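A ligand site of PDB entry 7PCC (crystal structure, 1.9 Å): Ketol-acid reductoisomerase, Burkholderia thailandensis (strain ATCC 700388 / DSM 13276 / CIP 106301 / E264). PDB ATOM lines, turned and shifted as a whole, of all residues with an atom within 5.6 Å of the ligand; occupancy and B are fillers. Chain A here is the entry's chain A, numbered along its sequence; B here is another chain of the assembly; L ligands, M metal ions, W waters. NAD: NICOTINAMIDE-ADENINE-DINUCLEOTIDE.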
ATOM      1  N   GLY A  25     -25.342 -17.181 -22.841  1.00  0.00           N
ATOM      2  CA  GLY A  25     -25.004 -16.913 -21.434  1.00  0.00           C
ATOM      3  C   GLY A  25     -26.168 -16.261 -20.721  1.00  0.00           C
ATOM      4  O   GLY A  25     -26.957 -15.551 -21.368  1.00  0.00           O
ATOM      5  N   TYR A  26     -26.280 -16.502 -19.419  1.00  0.00           N
ATOM      6  CA  TYR A  26     -27.386 -16.024 -18.572  1.00  0.00           C
ATOM      7  C   TYR A  26     -26.796 -15.622 -17.218  1.00  0.00           C
ATOM      8  O   TYR A  26     -27.403 -15.889 -16.166  1.00  0.00           O
ATOM      9  CB  TYR A  26     -28.468 -17.093 -18.497  1.00  0.00           C
ATOM     10  CG  TYR A  26     -29.813 -16.582 -18.056  1.00  0.00           C
ATOM     11  CD1 TYR A  26     -30.629 -15.854 -18.923  1.00  0.00           C
ATOM     12  CD2 TYR A  26     -30.268 -16.796 -16.771  1.00  0.00           C
ATOM     13  CE1 TYR A  26     -31.858 -15.380 -18.510  1.00  0.00           C
ATOM     14  CE2 TYR A  26     -31.506 -16.329 -16.349  1.00  0.00           C
ATOM     15  CZ  TYR A  26     -32.301 -15.622 -17.219  1.00  0.00           C
ATOM     16  OH  TYR A  26     -33.508 -15.160 -16.802  1.00  0.00           O
ATOM     17  N   GLY A  27     -25.613 -15.007 -17.260  1.00  0.00           N
ATOM     18  CA  GLY A  27     -24.888 -14.529 -16.073  1.00  0.00           C
ATOM     19  C   GLY A  27     -25.244 -13.095 -15.761  1.00  0.00           C
ATOM     20  O   GLY A  27     -26.413 -12.709 -15.975  1.00  0.00           O
ATOM     21  N   ILE A  28     -24.268 -12.324 -15.299  1.00  0.00           N
ATOM     22  CA  ILE A  28     -24.428 -10.917 -14.860  1.00  0.00           C
ATOM     23  C   ILE A  28     -25.063 -10.113 -16.005  1.00  0.00           C
ATOM     24  O   ILE A  28     -26.078  -9.434 -15.752  1.00  0.00           O
ATOM     25  CB  ILE A  28     -23.060 -10.365 -14.395  1.00  0.00           C
ATOM     26  CG1 ILE A  28     -22.570 -11.091 -13.145  1.00  0.00           C
ATOM     27  CG2 ILE A  28     -23.114  -8.858 -14.180  1.00  0.00           C
ATOM     28  CD1 ILE A  28     -21.064 -11.224 -13.046  1.00  0.00           C
ATOM     29  N   GLN A  29     -24.522 -10.211 -17.218  1.00  0.00           N
ATOM     30  CA  GLN A  29     -24.998  -9.467 -18.406  1.00  0.00           C
ATOM     31  C   GLN A  29     -26.152 -10.229 -19.071  1.00  0.00           C
ATOM     32  O   GLN A  29     -27.191  -9.590 -19.337  1.00  0.00           O
ATOM     33  CB  GLN A  29     -23.850  -9.223 -19.389  1.00  0.00           C
ATOM     34  CG  GLN A  29     -22.808  -8.236 -18.871  1.00  0.00           C
ATOM     35  CD  GLN A  29     -23.385  -6.866 -18.617  1.00  0.00           C
ATOM     36  OE1 GLN A  29     -24.218  -6.371 -19.369  1.00  0.00           O
ATOM     37  NE2 GLN A  29     -22.940  -6.236 -17.542  1.00  0.00           N
ATOM     38  N   GLY A  30     -25.985 -11.530 -19.311  1.00  0.00           N
ATOM     39  CA  GLY A  30     -26.945 -12.383 -20.053  1.00  0.00           C
ATOM     40  C   GLY A  30     -28.360 -12.274 -19.494  1.00  0.00           C
ATOM     41  O   GLY A  30     -29.311 -12.105 -20.280  1.00  0.00           O
ATOM     42  N   ASN A  48     -27.205 -21.802 -23.468  1.00  0.00           N
ATOM     43  CA  ASN A  48     -26.344 -21.944 -22.269  1.00  0.00           C
ATOM     44  C   ASN A  48     -25.813 -23.382 -22.178  1.00  0.00           C
ATOM     45  O   ASN A  48     -26.513 -24.302 -22.637  1.00  0.00           O
ATOM     46  CB  ASN A  48     -27.089 -21.522 -20.996  1.00  0.00           C
ATOM     47  CG  ASN A  48     -26.160 -21.017 -19.913  1.00  0.00           C
ATOM     48  OD1 ASN A  48     -25.915 -19.814 -19.817  1.00  0.00           O
ATOM     49  ND2 ASN A  48     -25.613 -21.924 -19.124  1.00  0.00           N
ATOM     50  N   ILE A  49     -24.629 -23.532 -21.599  1.00  0.00           N
ATOM     51  CA  ILE A  49     -24.026 -24.853 -21.241  1.00  0.00           C
ATOM     52  C   ILE A  49     -24.830 -25.448 -20.079  1.00  0.00           C
ATOM     53  O   ILE A  49     -25.724 -24.748 -19.554  1.00  0.00           O
ATOM     54  CB  ILE A  49     -22.519 -24.719 -20.927  1.00  0.00           C
ATOM     55  CG1 ILE A  49     -22.252 -23.737 -19.773  1.00  0.00           C
ATOM     56  CG2 ILE A  49     -21.748 -24.350 -22.176  1.00  0.00           C
ATOM     57  CD1 ILE A  49     -20.852 -23.802 -19.219  1.00  0.00           C
ATOM     58  N   ASP A  51     -25.210 -25.960 -16.734  1.00  0.00           N
ATOM     59  CA  ASP A  51     -24.802 -25.438 -15.392  1.00  0.00           C
ATOM     60  C   ASP A  51     -26.005 -24.744 -14.747  1.00  0.00           C
ATOM     61  O   ASP A  51     -27.108 -24.835 -15.302  1.00  0.00           O
ATOM     62  CB  ASP A  51     -23.560 -24.548 -15.496  1.00  0.00           C
ATOM     63  CG  ASP A  51     -23.778 -23.219 -16.206  1.00  0.00           C
ATOM     64  OD1 ASP A  51     -24.944 -22.852 -16.446  1.00  0.00           O
ATOM     65  OD2 ASP A  51     -22.765 -22.540 -16.510  1.00  0.00           O
ATOM     66  N   TYR A  53     -26.930 -21.701 -14.478  1.00  0.00           N
ATOM     67  CA  TYR A  53     -27.499 -20.562 -15.250  1.00  0.00           C
ATOM     68  C   TYR A  53     -28.565 -21.078 -16.242  1.00  0.00           C
ATOM     69  O   TYR A  53     -29.553 -20.363 -16.467  1.00  0.00           O
ATOM     70  CB  TYR A  53     -26.388 -19.792 -15.955  1.00  0.00           C
ATOM     71  CG  TYR A  53     -25.356 -19.191 -15.037  1.00  0.00           C
ATOM     72  CD1 TYR A  53     -24.166 -19.844 -14.756  1.00  0.00           C
ATOM     73  CD2 TYR A  53     -25.540 -17.937 -14.474  1.00  0.00           C
ATOM     74  CE1 TYR A  53     -23.194 -19.282 -13.951  1.00  0.00           C
ATOM     75  CE2 TYR A  53     -24.579 -17.360 -13.658  1.00  0.00           C
ATOM     76  CZ  TYR A  53     -23.406 -18.039 -13.396  1.00  0.00           C
ATOM     77  OH  TYR A  53     -22.463 -17.479 -12.593  1.00  0.00           O
ATOM     78  N   ILE A  67     -25.912 -23.880 -26.784  1.00  0.00           N
ATOM     79  CA  ILE A  67     -25.529 -22.627 -27.512  1.00  0.00           C
ATOM     80  C   ILE A  67     -25.777 -22.816 -29.010  1.00  0.00           C
ATOM     81  O   ILE A  67     -26.384 -21.920 -29.622  1.00  0.00           O
ATOM     82  CB  ILE A  67     -24.078 -22.240 -27.165  1.00  0.00           C
ATOM     83  CG1 ILE A  67     -23.960 -21.828 -25.692  1.00  0.00           C
ATOM     84  CG2 ILE A  67     -23.565 -21.155 -28.099  1.00  0.00           C
ATOM     85  CD1 ILE A  67     -22.546 -21.683 -25.186  1.00  0.00           C
ATOM     86  N   LEU A  79     -23.177 -12.621 -27.404  1.00  0.00           N
ATOM     87  CA  LEU A  79     -22.186 -13.540 -26.772  1.00  0.00           C
ATOM     88  C   LEU A  79     -21.823 -12.988 -25.396  1.00  0.00           C
ATOM     89  O   LEU A  79     -20.823 -12.246 -25.286  1.00  0.00           O
ATOM     90  CB  LEU A  79     -20.968 -13.668 -27.688  1.00  0.00           C
ATOM     91  CG  LEU A  79     -19.881 -14.637 -27.227  1.00  0.00           C
ATOM     92  CD1 LEU A  79     -20.484 -15.988 -26.838  1.00  0.00           C
ATOM     93  CD2 LEU A  79     -18.810 -14.809 -28.285  1.00  0.00           C
ATOM     94  N   LEU A  80     -22.632 -13.334 -24.376  1.00  0.00           N
ATOM     95  CA  LEU A  80     -22.519 -12.808 -22.994  1.00  0.00           C
ATOM     96  C   LEU A  80     -22.042 -13.927 -22.061  1.00  0.00           C
ATOM     97  O   LEU A  80     -22.758 -14.260 -21.093  1.00  0.00           O
ATOM     98  CB  LEU A  80     -23.877 -12.230 -22.579  1.00  0.00           C
ATOM     99  CG  LEU A  80     -24.397 -11.103 -23.481  1.00  0.00           C
ATOM    100  CD1 LEU A  80     -25.753 -10.605 -22.988  1.00  0.00           C
ATOM    101  CD2 LEU A  80     -23.413  -9.942 -23.564  1.00  0.00           C
ATOM    102  N   ILE A  81     -20.873 -14.481 -22.373  1.00  0.00           N
ATOM    103  CA  ILE A  81     -20.111 -15.464 -21.540  1.00  0.00           C
ATOM    104  C   ILE A  81     -18.719 -14.901 -21.312  1.00  0.00           C
ATOM    105  O   ILE A  81     -18.336 -13.921 -21.953  1.00  0.00           O
ATOM    106  CB  ILE A  81     -20.078 -16.846 -22.231  1.00  0.00           C
ATOM    107  CG1 ILE A  81     -19.183 -16.848 -23.474  1.00  0.00           C
ATOM    108  CG2 ILE A  81     -21.493 -17.325 -22.545  1.00  0.00           C
ATOM    109  CD1 ILE A  81     -18.937 -18.209 -24.065  1.00  0.00           C
ATOM    110  N   PRO A  82     -17.922 -15.460 -20.374  1.00  0.00           N
ATOM    111  CA  PRO A  82     -16.552 -14.997 -20.132  1.00  0.00           C
ATOM    112  C   PRO A  82     -15.679 -14.953 -21.392  1.00  0.00           C
ATOM    113  O   PRO A  82     -15.754 -15.853 -22.206  1.00  0.00           O
ATOM    114  CB  PRO A  82     -16.009 -16.017 -19.116  1.00  0.00           C
ATOM    115  CG  PRO A  82     -17.243 -16.459 -18.373  1.00  0.00           C
ATOM    116  CD  PRO A  82     -18.317 -16.520 -19.434  1.00  0.00           C
ATOM    117  N   ASP A  83     -14.844 -13.920 -21.480  1.00  0.00           N
ATOM    118  CA  ASP A  83     -14.065 -13.546 -22.701  1.00  0.00           C
ATOM    119  C   ASP A  83     -13.128 -14.695 -23.092  1.00  0.00           C
ATOM    120  O   ASP A  83     -12.997 -14.934 -24.307  1.00  0.00           O
ATOM    121  CB  ASP A  83     -13.318 -12.234 -22.454  1.00  0.00           C
ATOM    122  CG  ASP A  83     -14.245 -11.119 -22.013  1.00  0.00           C
ATOM    123  OD1 ASP A  83     -15.068 -10.680 -22.841  1.00  0.00           O
ATOM    124  OD2 ASP A  83     -14.177 -10.732 -20.828  1.00  0.00           O
ATOM    125  N   ALA A  85     -13.639 -17.787 -22.878  1.00  0.00           N
ATOM    126  CA  ALA A  85     -14.488 -18.866 -23.437  1.00  0.00           C
ATOM    127  C   ALA A  85     -14.962 -18.522 -24.861  1.00  0.00           C
ATOM    128  O   ALA A  85     -15.540 -19.422 -25.514  1.00  0.00           O
ATOM    129  CB  ALA A  85     -15.651 -19.121 -22.511  1.00  0.00           C
ATOM    130  N   HIS A  86     -14.733 -17.296 -25.338  1.00  0.00           N
ATOM    131  CA  HIS A  86     -15.219 -16.783 -26.654  1.00  0.00           C
ATOM    132  C   HIS A  86     -14.634 -17.623 -27.807  1.00  0.00           C
ATOM    133  O   HIS A  86     -15.406 -18.022 -28.680  1.00  0.00           O
ATOM    134  CB  HIS A  86     -14.904 -15.291 -26.831  1.00  0.00           C
ATOM    135  CG  HIS A  86     -15.793 -14.389 -26.050  1.00  0.00           C
ATOM    136  ND1 HIS A  86     -15.986 -13.053 -26.399  1.00  0.00           N
ATOM    137  CD2 HIS A  86     -16.558 -14.604 -24.962  1.00  0.00           C
ATOM    138  CE1 HIS A  86     -16.818 -12.494 -25.544  1.00  0.00           C
ATOM    139  NE2 HIS A  86     -17.181 -13.429 -24.651  1.00  0.00           N
ATOM    140  N   VAL A  89     -16.121 -21.352 -28.069  1.00  0.00           N
ATOM    141  CA  VAL A  89     -17.597 -21.237 -28.292  1.00  0.00           C
ATOM    142  C   VAL A  89     -17.835 -20.632 -29.690  1.00  0.00           C
ATOM    143  O   VAL A  89     -18.754 -21.090 -30.371  1.00  0.00           O
ATOM    144  CB  VAL A  89     -18.307 -20.437 -27.179  1.00  0.00           C
ATOM    145  CG1 VAL A  89     -19.761 -20.153 -27.514  1.00  0.00           C
ATOM    146  CG2 VAL A  89     -18.214 -21.166 -25.845  1.00  0.00           C
ATOM    147  N   ALA A 107     -19.987  -7.823 -25.743  1.00  0.00           N
ATOM    148  CA  ALA A 107     -20.203  -6.726 -24.776  1.00  0.00           C
ATOM    149  C   ALA A 107     -18.868  -6.205 -24.223  1.00  0.00           C
ATOM    150  O   ALA A 107     -18.892  -5.412 -23.276  1.00  0.00           O
ATOM    151  CB  ALA A 107     -21.126  -7.190 -23.681  1.00  0.00           C
ATOM    152  N   HIS A 108     -17.752  -6.628 -24.834  1.00  0.00           N
ATOM    153  CA  HIS A 108     -16.360  -6.289 -24.447  1.00  0.00           C
ATOM    154  C   HIS A 108     -15.452  -6.556 -25.646  1.00  0.00           C
ATOM    155  O   HIS A 108     -15.696  -7.565 -26.341  1.00  0.00           O
ATOM    156  CB  HIS A 108     -15.974  -7.086 -23.186  1.00  0.00           C
ATOM    157  CG  HIS A 108     -14.619  -6.781 -22.639  1.00  0.00           C
ATOM    158  ND1 HIS A 108     -14.060  -5.523 -22.664  1.00  0.00           N
ATOM    159  CD2 HIS A 108     -13.731  -7.576 -21.992  1.00  0.00           C
ATOM    160  CE1 HIS A 108     -12.878  -5.550 -22.084  1.00  0.00           C
ATOM    161  NE2 HIS A 108     -12.658  -6.798 -21.660  1.00  0.00           N
ATOM    162  N   ALA A 129     -21.189  -2.548 -25.503  1.00  0.00           N
ATOM    163  CA  ALA A 129     -20.471  -2.723 -24.217  1.00  0.00           C
ATOM    164  C   ALA A 129     -21.105  -1.844 -23.147  1.00  0.00           C
ATOM    165  O   ALA A 129     -20.808  -0.650 -23.081  1.00  0.00           O
ATOM    166  CB  ALA A 129     -19.008  -2.400 -24.419  1.00  0.00           C
ATOM    167  N   PRO A 130     -21.984  -2.402 -22.277  1.00  0.00           N
ATOM    168  CA  PRO A 130     -22.561  -1.627 -21.171  1.00  0.00           C
ATOM    169  C   PRO A 130     -21.493  -1.116 -20.206  1.00  0.00           C
ATOM    170  O   PRO A 130     -20.515  -1.826 -19.990  1.00  0.00           O
ATOM    171  CB  PRO A 130     -23.480  -2.624 -20.456  1.00  0.00           C
ATOM    172  CG  PRO A 130     -23.736  -3.717 -21.468  1.00  0.00           C
ATOM    173  CD  PRO A 130     -22.478  -3.780 -22.314  1.00  0.00           C
ATOM    174  N   MET A 132     -21.925  -0.745 -17.017  1.00  0.00           N
ATOM    175  CA  MET A 132     -22.659  -1.082 -15.770  1.00  0.00           C
ATOM    176  C   MET A 132     -22.823  -2.602 -15.699  1.00  0.00           C
ATOM    177  O   MET A 132     -22.836  -3.232 -16.775  1.00  0.00           O
ATOM    178  CB  MET A 132     -24.031  -0.395 -15.769  1.00  0.00           C
ATOM    179  CG  MET A 132     -24.790  -0.494 -14.462  1.00  0.00           C
ATOM    180  SD  MET A 132     -23.912   0.223 -13.043  1.00  0.00           S
ATOM    181  CE  MET A 132     -23.883   1.953 -13.504  1.00  0.00           C
ATOM    182  N   TYR A 133     -22.951  -3.153 -14.483  1.00  0.00           N
ATOM    183  CA  TYR A 133     -23.233  -4.600 -14.262  1.00  0.00           C
ATOM    184  C   TYR A 133     -24.755  -4.803 -14.256  1.00  0.00           C
ATOM    185  O   TYR A 133     -25.503  -3.820 -14.376  1.00  0.00           O
ATOM    186  CB  TYR A 133     -22.489  -5.127 -13.030  1.00  0.00           C
ATOM    187  CG  TYR A 133     -22.604  -4.356 -11.743  1.00  0.00           C
ATOM    188  CD1 TYR A 133     -23.550  -4.688 -10.786  1.00  0.00           C
ATOM    189  CD2 TYR A 133     -21.722  -3.333 -11.445  1.00  0.00           C
ATOM    190  CE1 TYR A 133     -23.640  -4.015  -9.581  1.00  0.00           C
ATOM    191  CE2 TYR A 133     -21.793  -2.639 -10.249  1.00  0.00           C
ATOM    192  CZ  TYR A 133     -22.748  -2.982  -9.313  1.00  0.00           C
ATOM    193  OH  TYR A 133     -22.817  -2.298  -8.137  1.00  0.00           O
ATOM    194  N   GLY A 134     -25.187  -6.065 -14.149  1.00  0.00           N
ATOM    195  CA  GLY A 134     -26.540  -6.526 -14.512  1.00  0.00           C
ATOM    196  C   GLY A 134     -27.646  -5.945 -13.653  1.00  0.00           C
ATOM    197  O   GLY A 134     -28.614  -5.412 -14.242  1.00  0.00           O
ATOM    198  N   ASP A 191     -11.754  -0.450 -20.192  1.00  0.00           N
ATOM    199  CA  ASP A 191     -12.516  -1.397 -19.343  1.00  0.00           C
ATOM    200  C   ASP A 191     -11.531  -2.130 -18.418  1.00  0.00           C
ATOM    201  O   ASP A 191     -11.786  -2.175 -17.209  1.00  0.00           O
ATOM    202  CB  ASP A 191     -13.337  -2.347 -20.216  1.00  0.00           C
ATOM    203  CG  ASP A 191     -14.380  -3.129 -19.445  1.00  0.00           C
ATOM    204  OD1 ASP A 191     -15.355  -2.497 -18.980  1.00  0.00           O
ATOM    205  OD2 ASP A 191     -14.194  -4.358 -19.315  1.00  0.00           O
ATOM    206  N   GLU B 232     -20.824   3.574 -12.095  1.00  0.00           N
ATOM    207  CA  GLU B 232     -20.426   2.164 -11.861  1.00  0.00           C
ATOM    208  C   GLU B 232     -19.552   2.069 -10.604  1.00  0.00           C
ATOM    209  O   GLU B 232     -19.825   1.180  -9.776  1.00  0.00           O
ATOM    210  CB  GLU B 232     -19.691   1.606 -13.084  1.00  0.00           C
ATOM    211  CG  GLU B 232     -19.446   0.114 -13.006  1.00  0.00           C
ATOM    212  CD  GLU B 232     -19.109  -0.532 -14.340  1.00  0.00           C
ATOM    213  OE1 GLU B 232     -18.390   0.095 -15.147  1.00  0.00           O
ATOM    214  OE2 GLU B 232     -19.580  -1.671 -14.586  1.00  0.00           O
ATOM    215  N   GLN B 252     -20.509  -9.606  -9.019  1.00  0.00           N
ATOM    216  CA  GLN B 252     -20.929  -8.741 -10.157  1.00  0.00           C
ATOM    217  C   GLN B 252     -19.807  -8.604 -11.204  1.00  0.00           C
ATOM    218  O   GLN B 252     -20.085  -8.023 -12.263  1.00  0.00           O
ATOM    219  CB  GLN B 252     -21.312  -7.348  -9.654  1.00  0.00           C
ATOM    220  CG  GLN B 252     -22.388  -7.348  -8.583  1.00  0.00           C
ATOM    221  CD  GLN B 252     -23.743  -7.779  -9.109  1.00  0.00           C
ATOM    222  OE1 GLN B 252     -23.869  -8.399 -10.153  1.00  0.00           O
ATOM    223  NE2 GLN B 252     -24.779  -7.448  -8.355  1.00  0.00           N
ATOM    224  N   GLY B 253     -18.594  -9.074 -10.915  1.00  0.00           N
ATOM    225  CA  GLY B 253     -17.455  -8.995 -11.844  1.00  0.00           C
ATOM    226  C   GLY B 253     -17.434 -10.189 -12.782  1.00  0.00           C
ATOM    227  O   GLY B 253     -17.550 -11.338 -12.287  1.00  0.00           O
ATOM    228  N   SER B 254     -17.281  -9.953 -14.088  1.00  0.00           N
ATOM    229  CA  SER B 254     -16.908 -11.004 -15.072  1.00  0.00           C
ATOM    230  C   SER B 254     -15.620 -11.665 -14.587  1.00  0.00           C
ATOM    231  O   SER B 254     -14.860 -11.046 -13.852  1.00  0.00           O
ATOM    232  CB  SER B 254     -16.722 -10.426 -16.453  1.00  0.00           C
ATOM    233  OG  SER B 254     -15.443  -9.810 -16.581  1.00  0.00           O
ATOM    234  N   PRO B 255     -15.316 -12.924 -14.982  1.00  0.00           N
ATOM    235  CA  PRO B 255     -14.045 -13.541 -14.614  1.00  0.00           C
ATOM    236  C   PRO B 255     -12.836 -12.697 -15.058  1.00  0.00           C
ATOM    237  O   PRO B 255     -11.888 -12.604 -14.294  1.00  0.00           O
ATOM    238  CB  PRO B 255     -14.094 -14.891 -15.331  1.00  0.00           C
ATOM    239  CG  PRO B 255     -15.568 -15.178 -15.460  1.00  0.00           C
ATOM    240  CD  PRO B 255     -16.168 -13.812 -15.774  1.00  0.00           C
ATOM    241  N   THR B 256     -12.895 -12.100 -16.254  1.00  0.00           N
ATOM    242  CA  THR B 256     -11.851 -11.174 -16.775  1.00  0.00           C
ATOM    243  C   THR B 256     -11.619 -10.053 -15.754  1.00  0.00           C
ATOM    244  O   THR B 256     -10.447  -9.804 -15.406  1.00  0.00           O
ATOM    245  CB  THR B 256     -12.240 -10.589 -18.138  1.00  0.00           C
ATOM    246  OG1 THR B 256     -12.474 -11.675 -19.035  1.00  0.00           O
ATOM    247  CG2 THR B 256     -11.181  -9.672 -18.714  1.00  0.00           C
HETATM  248  PA  NAD L   1     -20.556 -14.256 -15.923  1.00  0.00           P
HETATM  249  O1A NAD L   1     -19.404 -14.758 -15.116  1.00  0.00           O
HETATM  250  O2A NAD L   1     -21.801 -13.818 -15.202  1.00  0.00           O
HETATM  251  O5B NAD L   1     -20.937 -15.339 -17.026  1.00  0.00           O
HETATM  252  C5B NAD L   1     -21.613 -16.554 -16.651  1.00  0.00           C
HETATM  253  C4B NAD L   1     -22.331 -17.092 -17.856  1.00  0.00           C
HETATM  254  O4B NAD L   1     -21.347 -17.584 -18.811  1.00  0.00           O
HETATM  255  C3B NAD L   1     -23.284 -18.265 -17.611  1.00  0.00           C
HETATM  256  O3B NAD L   1     -24.377 -18.215 -18.519  1.00  0.00           O
HETATM  257  C2B NAD L   1     -22.370 -19.470 -17.858  1.00  0.00           C
HETATM  258  O2B NAD L   1     -23.096 -20.630 -18.193  1.00  0.00           O
HETATM  259  C1B NAD L   1     -21.557 -18.957 -19.042  1.00  0.00           C
HETATM  260  N9A NAD L   1     -20.267 -19.607 -19.213  1.00  0.00           N
HETATM  261  C8A NAD L   1     -19.216 -19.616 -18.337  1.00  0.00           C
HETATM  262  N7A NAD L   1     -18.180 -20.283 -18.777  1.00  0.00           N
HETATM  263  C5A NAD L   1     -18.569 -20.743 -20.027  1.00  0.00           C
HETATM  264  C6A NAD L   1     -17.911 -21.511 -21.006  1.00  0.00           C
HETATM  265  N6A NAD L   1     -16.669 -21.982 -20.865  1.00  0.00           N
HETATM  266  N1A NAD L   1     -18.596 -21.797 -22.142  1.00  0.00           N
HETATM  267  C2A NAD L   1     -19.839 -21.332 -22.274  1.00  0.00           C
HETATM  268  N3A NAD L   1     -20.556 -20.591 -21.425  1.00  0.00           N
HETATM  269  C4A NAD L   1     -19.858 -20.328 -20.306  1.00  0.00           C
HETATM  270  O3  NAD L   1     -20.029 -13.094 -16.876  1.00  0.00           O
HETATM  271  PN  NAD L   1     -20.530 -11.638 -17.298  1.00  0.00           P
HETATM  272  O1N NAD L   1     -20.032 -10.656 -16.291  1.00  0.00           O
HETATM  273  O2N NAD L   1     -21.996 -11.680 -17.595  1.00  0.00           O
HETATM  274  O5D NAD L   1     -19.705 -11.443 -18.659  1.00  0.00           O
HETATM  275  C5D NAD L   1     -20.241 -11.821 -19.948  1.00  0.00           C
HETATM  276  C4D NAD L   1     -19.654 -10.916 -20.998  1.00  0.00           C
HETATM  277  O4D NAD L   1     -20.127  -9.574 -20.752  1.00  0.00           O
HETATM  278  C3D NAD L   1     -18.121 -10.817 -21.028  1.00  0.00           C
HETATM  279  O3D NAD L   1     -17.670 -10.632 -22.359  1.00  0.00           O
HETATM  280  C2D NAD L   1     -17.869  -9.595 -20.145  1.00  0.00           C
HETATM  281  O2D NAD L   1     -16.614  -8.970 -20.377  1.00  0.00           O
HETATM  282  C1D NAD L   1     -19.010  -8.695 -20.606  1.00  0.00           C
HETATM  283  N1N NAD L   1     -19.367  -7.589 -19.644  1.00  0.00           N
HETATM  284  C2N NAD L   1     -19.446  -7.794 -18.280  1.00  0.00           C
HETATM  285  C3N NAD L   1     -19.732  -6.715 -17.423  1.00  0.00           C
HETATM  286  C7N NAD L   1     -19.921  -6.909 -15.940  1.00  0.00           C
HETATM  287  O7N NAD L   1     -20.139  -5.922 -15.235  1.00  0.00           O
HETATM  288  N7N NAD L   1     -19.858  -8.138 -15.453  1.00  0.00           N
HETATM  289  C4N NAD L   1     -19.856  -5.431 -17.981  1.00  0.00           C
HETATM  290  C5N NAD L   1     -19.933  -5.282 -19.349  1.00  0.00           C
HETATM  291  C6N NAD L   1     -19.639  -6.354 -20.163  1.00  0.00           C
HETATM  292 MG    MG M   1     -16.844  -2.602 -17.442  1.00  0.00          MG
HETATM  293 MG    MG M   2     -15.105  -5.766 -18.143  1.00  0.00          MG
HETATM  294  O   HOH W   1     -16.570  -4.796 -17.571  1.00  0.00           O
HETATM  295  O   HOH W   2     -18.421 -13.972 -12.924  1.00  0.00           O
HETATM  296  O   HOH W   3     -15.611 -19.568 -17.978  1.00  0.00           O
HETATM  297  O   HOH W   4     -14.736 -22.936 -23.085  1.00  0.00           O
HETATM  298  O   HOH W   5     -17.149  -4.433 -21.451  1.00  0.00           O
HETATM  299  O   HOH W   6     -16.222  -6.343 -19.806  1.00  0.00           O
HETATM  300  O   HOH W   7     -17.073  -6.597 -14.679  1.00  0.00           O
HETATM  301  O   HOH W   8     -18.527  -2.829 -16.447  1.00  0.00           O
HETATM  302  O   HOH W   9     -18.761 -17.604 -15.195  1.00  0.00           O
HETATM  303  O   HOH W  10     -19.139 -10.285 -24.726  1.00  0.00           O
HETATM  304  O   HOH W  11     -23.821 -13.326 -18.902  1.00  0.00           O
HETATM  305  O   HOH W  12     -18.875 -24.069 -23.898  1.00  0.00           O
HETATM  306  O   HOH W  13     -22.476 -14.795 -12.839  1.00  0.00           O
HETATM  307  O   HOH W  14     -18.030  -2.687 -19.356  1.00  0.00           O
HETATM  308  O   HOH W  15     -23.366 -20.768 -21.448  1.00  0.00           O
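The backbone NH (N) of Ser 254 of chain B lies close to a nitrogen (N7N) of the ligand (3.4 Å). CA of Gly 25 touches O3B of the ligand, at 3.3 Å. Gly 27 touches the ligand (CA to O2A, 3.3 Å). Ile 49 touches the ligand. CD1 of Tyr 53 touches C3B of the ligand, at 3.4 Å. CD1 of Ile 67 touches C2A of the ligand, at 3.99 Å. C of Leu 80 touches C5D of the ligand, at 3.5 Å. Pro 82 touches the ligand (CD to O4B, 3.3 Å). CB of Ala 85 touches N6A of the ligand, at 3.5 Å. His 86 touches the ligand. Val 89 touches the ligand (CG2 to N1A, 3.8 Å). Ala 107 touches the ligand. CB of His 108 touches O2D of the ligand, at 3.4 Å. O of Pro 130 touches C5N of the ligand (3.6 Å). Met 132 touches the ligand. Tyr 133 touches the ligand. Pro 255 of chain B touches the ligand (CD to O1A, 3.4 Å). Hydrophobic or aromatic side chains that line the ligand: Ile 28, Ile 49, Tyr 53, Ile 67, Ile 81, Pro 82, Ala 85, His 86, Val 89, Ala 107, His 108, Tyr 133 and Pro 255 of chain B. 25 residues have an atom within 4 Å of the ligand: Gly 25, Tyr 26, Gly 27, Ile 28, Gln 29, Asn 48, Ile 49, Asp 51, Tyr 53, Ile 67, Leu 80, Ile 81, Pro 82, Asp 83, Ala 85, His 86, Val 89, Ala 107, His 108, Pro 130, Met 132, Tyr 133, Gln 252 of chain B, Ser 254 of chain B and Pro 255 of chain B.
The side-chain amide nitrogen of Asn 48 sits at hydrogen-bond distance from the side-chain carboxylate of Asp 51. N of Tyr 53 lies within hydrogen-bond range of OD1 of Asp 51 (3.0 Å). The side-chain amide oxygen (OD1) of Asn 48 lies within hydrogen-bond range of the backbone NH (N) of Tyr 26 (3.4 Å). OG1 of Thr 256 of chain B is in hydrogen-bond range of OD2 of Asp 83 (2.6 Å). The side-chain amide nitrogen (NE2) of Gln 29 lies within hydrogen-bond range of the backbone carbonyl oxygen (O) of Met 132, 3.1 Å away. O of Ile 81 is in hydrogen-bond range of NE2 of His 86, at 3.0 Å. The backbone NH (N) of Thr 256 of chain B sits close to the side-chain hydroxyl (OG) of Ser 254 of chain B (3.4 Å).
The side-chain carboxylate (OD2) of Asp 51 sits at hydrogen-bond distance from an oxygen (O2B) of the ligand, at 2.6 Å. OD1 of Asn 48 is in hydrogen-bond range of O3B of the ligand (2.6 Å). The side-chain carboxylate of Asp 83 is in hydrogen-bond range of an oxygen (O3D) of the ligand, 2.6 Å away. The backbone NH of Tyr 26 is in hydrogen-bond range of an oxygen (O3B) of the ligand (2.7 Å). N of Ile 28 sits at hydrogen-bond distance from O2A of the ligand, at 2.9 Å. An oxygen (O2N) of the ligand is in hydrogen-bond range of the backbone NH (N) of Gln 29, 2.9 Å away. The backbone carbonyl oxygen of Gln 252 of chain B is in hydrogen-bond range of a nitrogen (N7N) of the ligand (3.2 Å). The backbone carbonyl oxygen (O) of Ile 81 lies close to an oxygen (O3D) of the ligand (3.4 Å).
Water W13 lies within hydrogen-bond range of O2A of the ligand (2.6 Å) and OH of Tyr 53 (2.7 Å). Water W11 lies within hydrogen-bond range of O of Leu 80, O2N of the ligand, N of Gly 30 and N of Gly 27. Water W10 lies within hydrogen-bond range of the backbone carbonyl oxygen (O) of Leu 79, the backbone NH (N) of Ala 107 and an oxygen (O3D) of the ligand. Water W15 lies within hydrogen-bond range of N3A of the ligand (2.8 Å), N of Ile 49 (3.0 Å) and OD1 of Asn 48 (3.2 Å). Water W7 lies within hydrogen-bond range of O7N of the ligand (3.2 Å) and N of Ser 254 of chain B (3.4 Å). Water W5 bridges the backbone carbonyl oxygen of Ala 107 (2.7 Å) and a ring nitrogen (ND1) of His 108 (3.5 Å).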
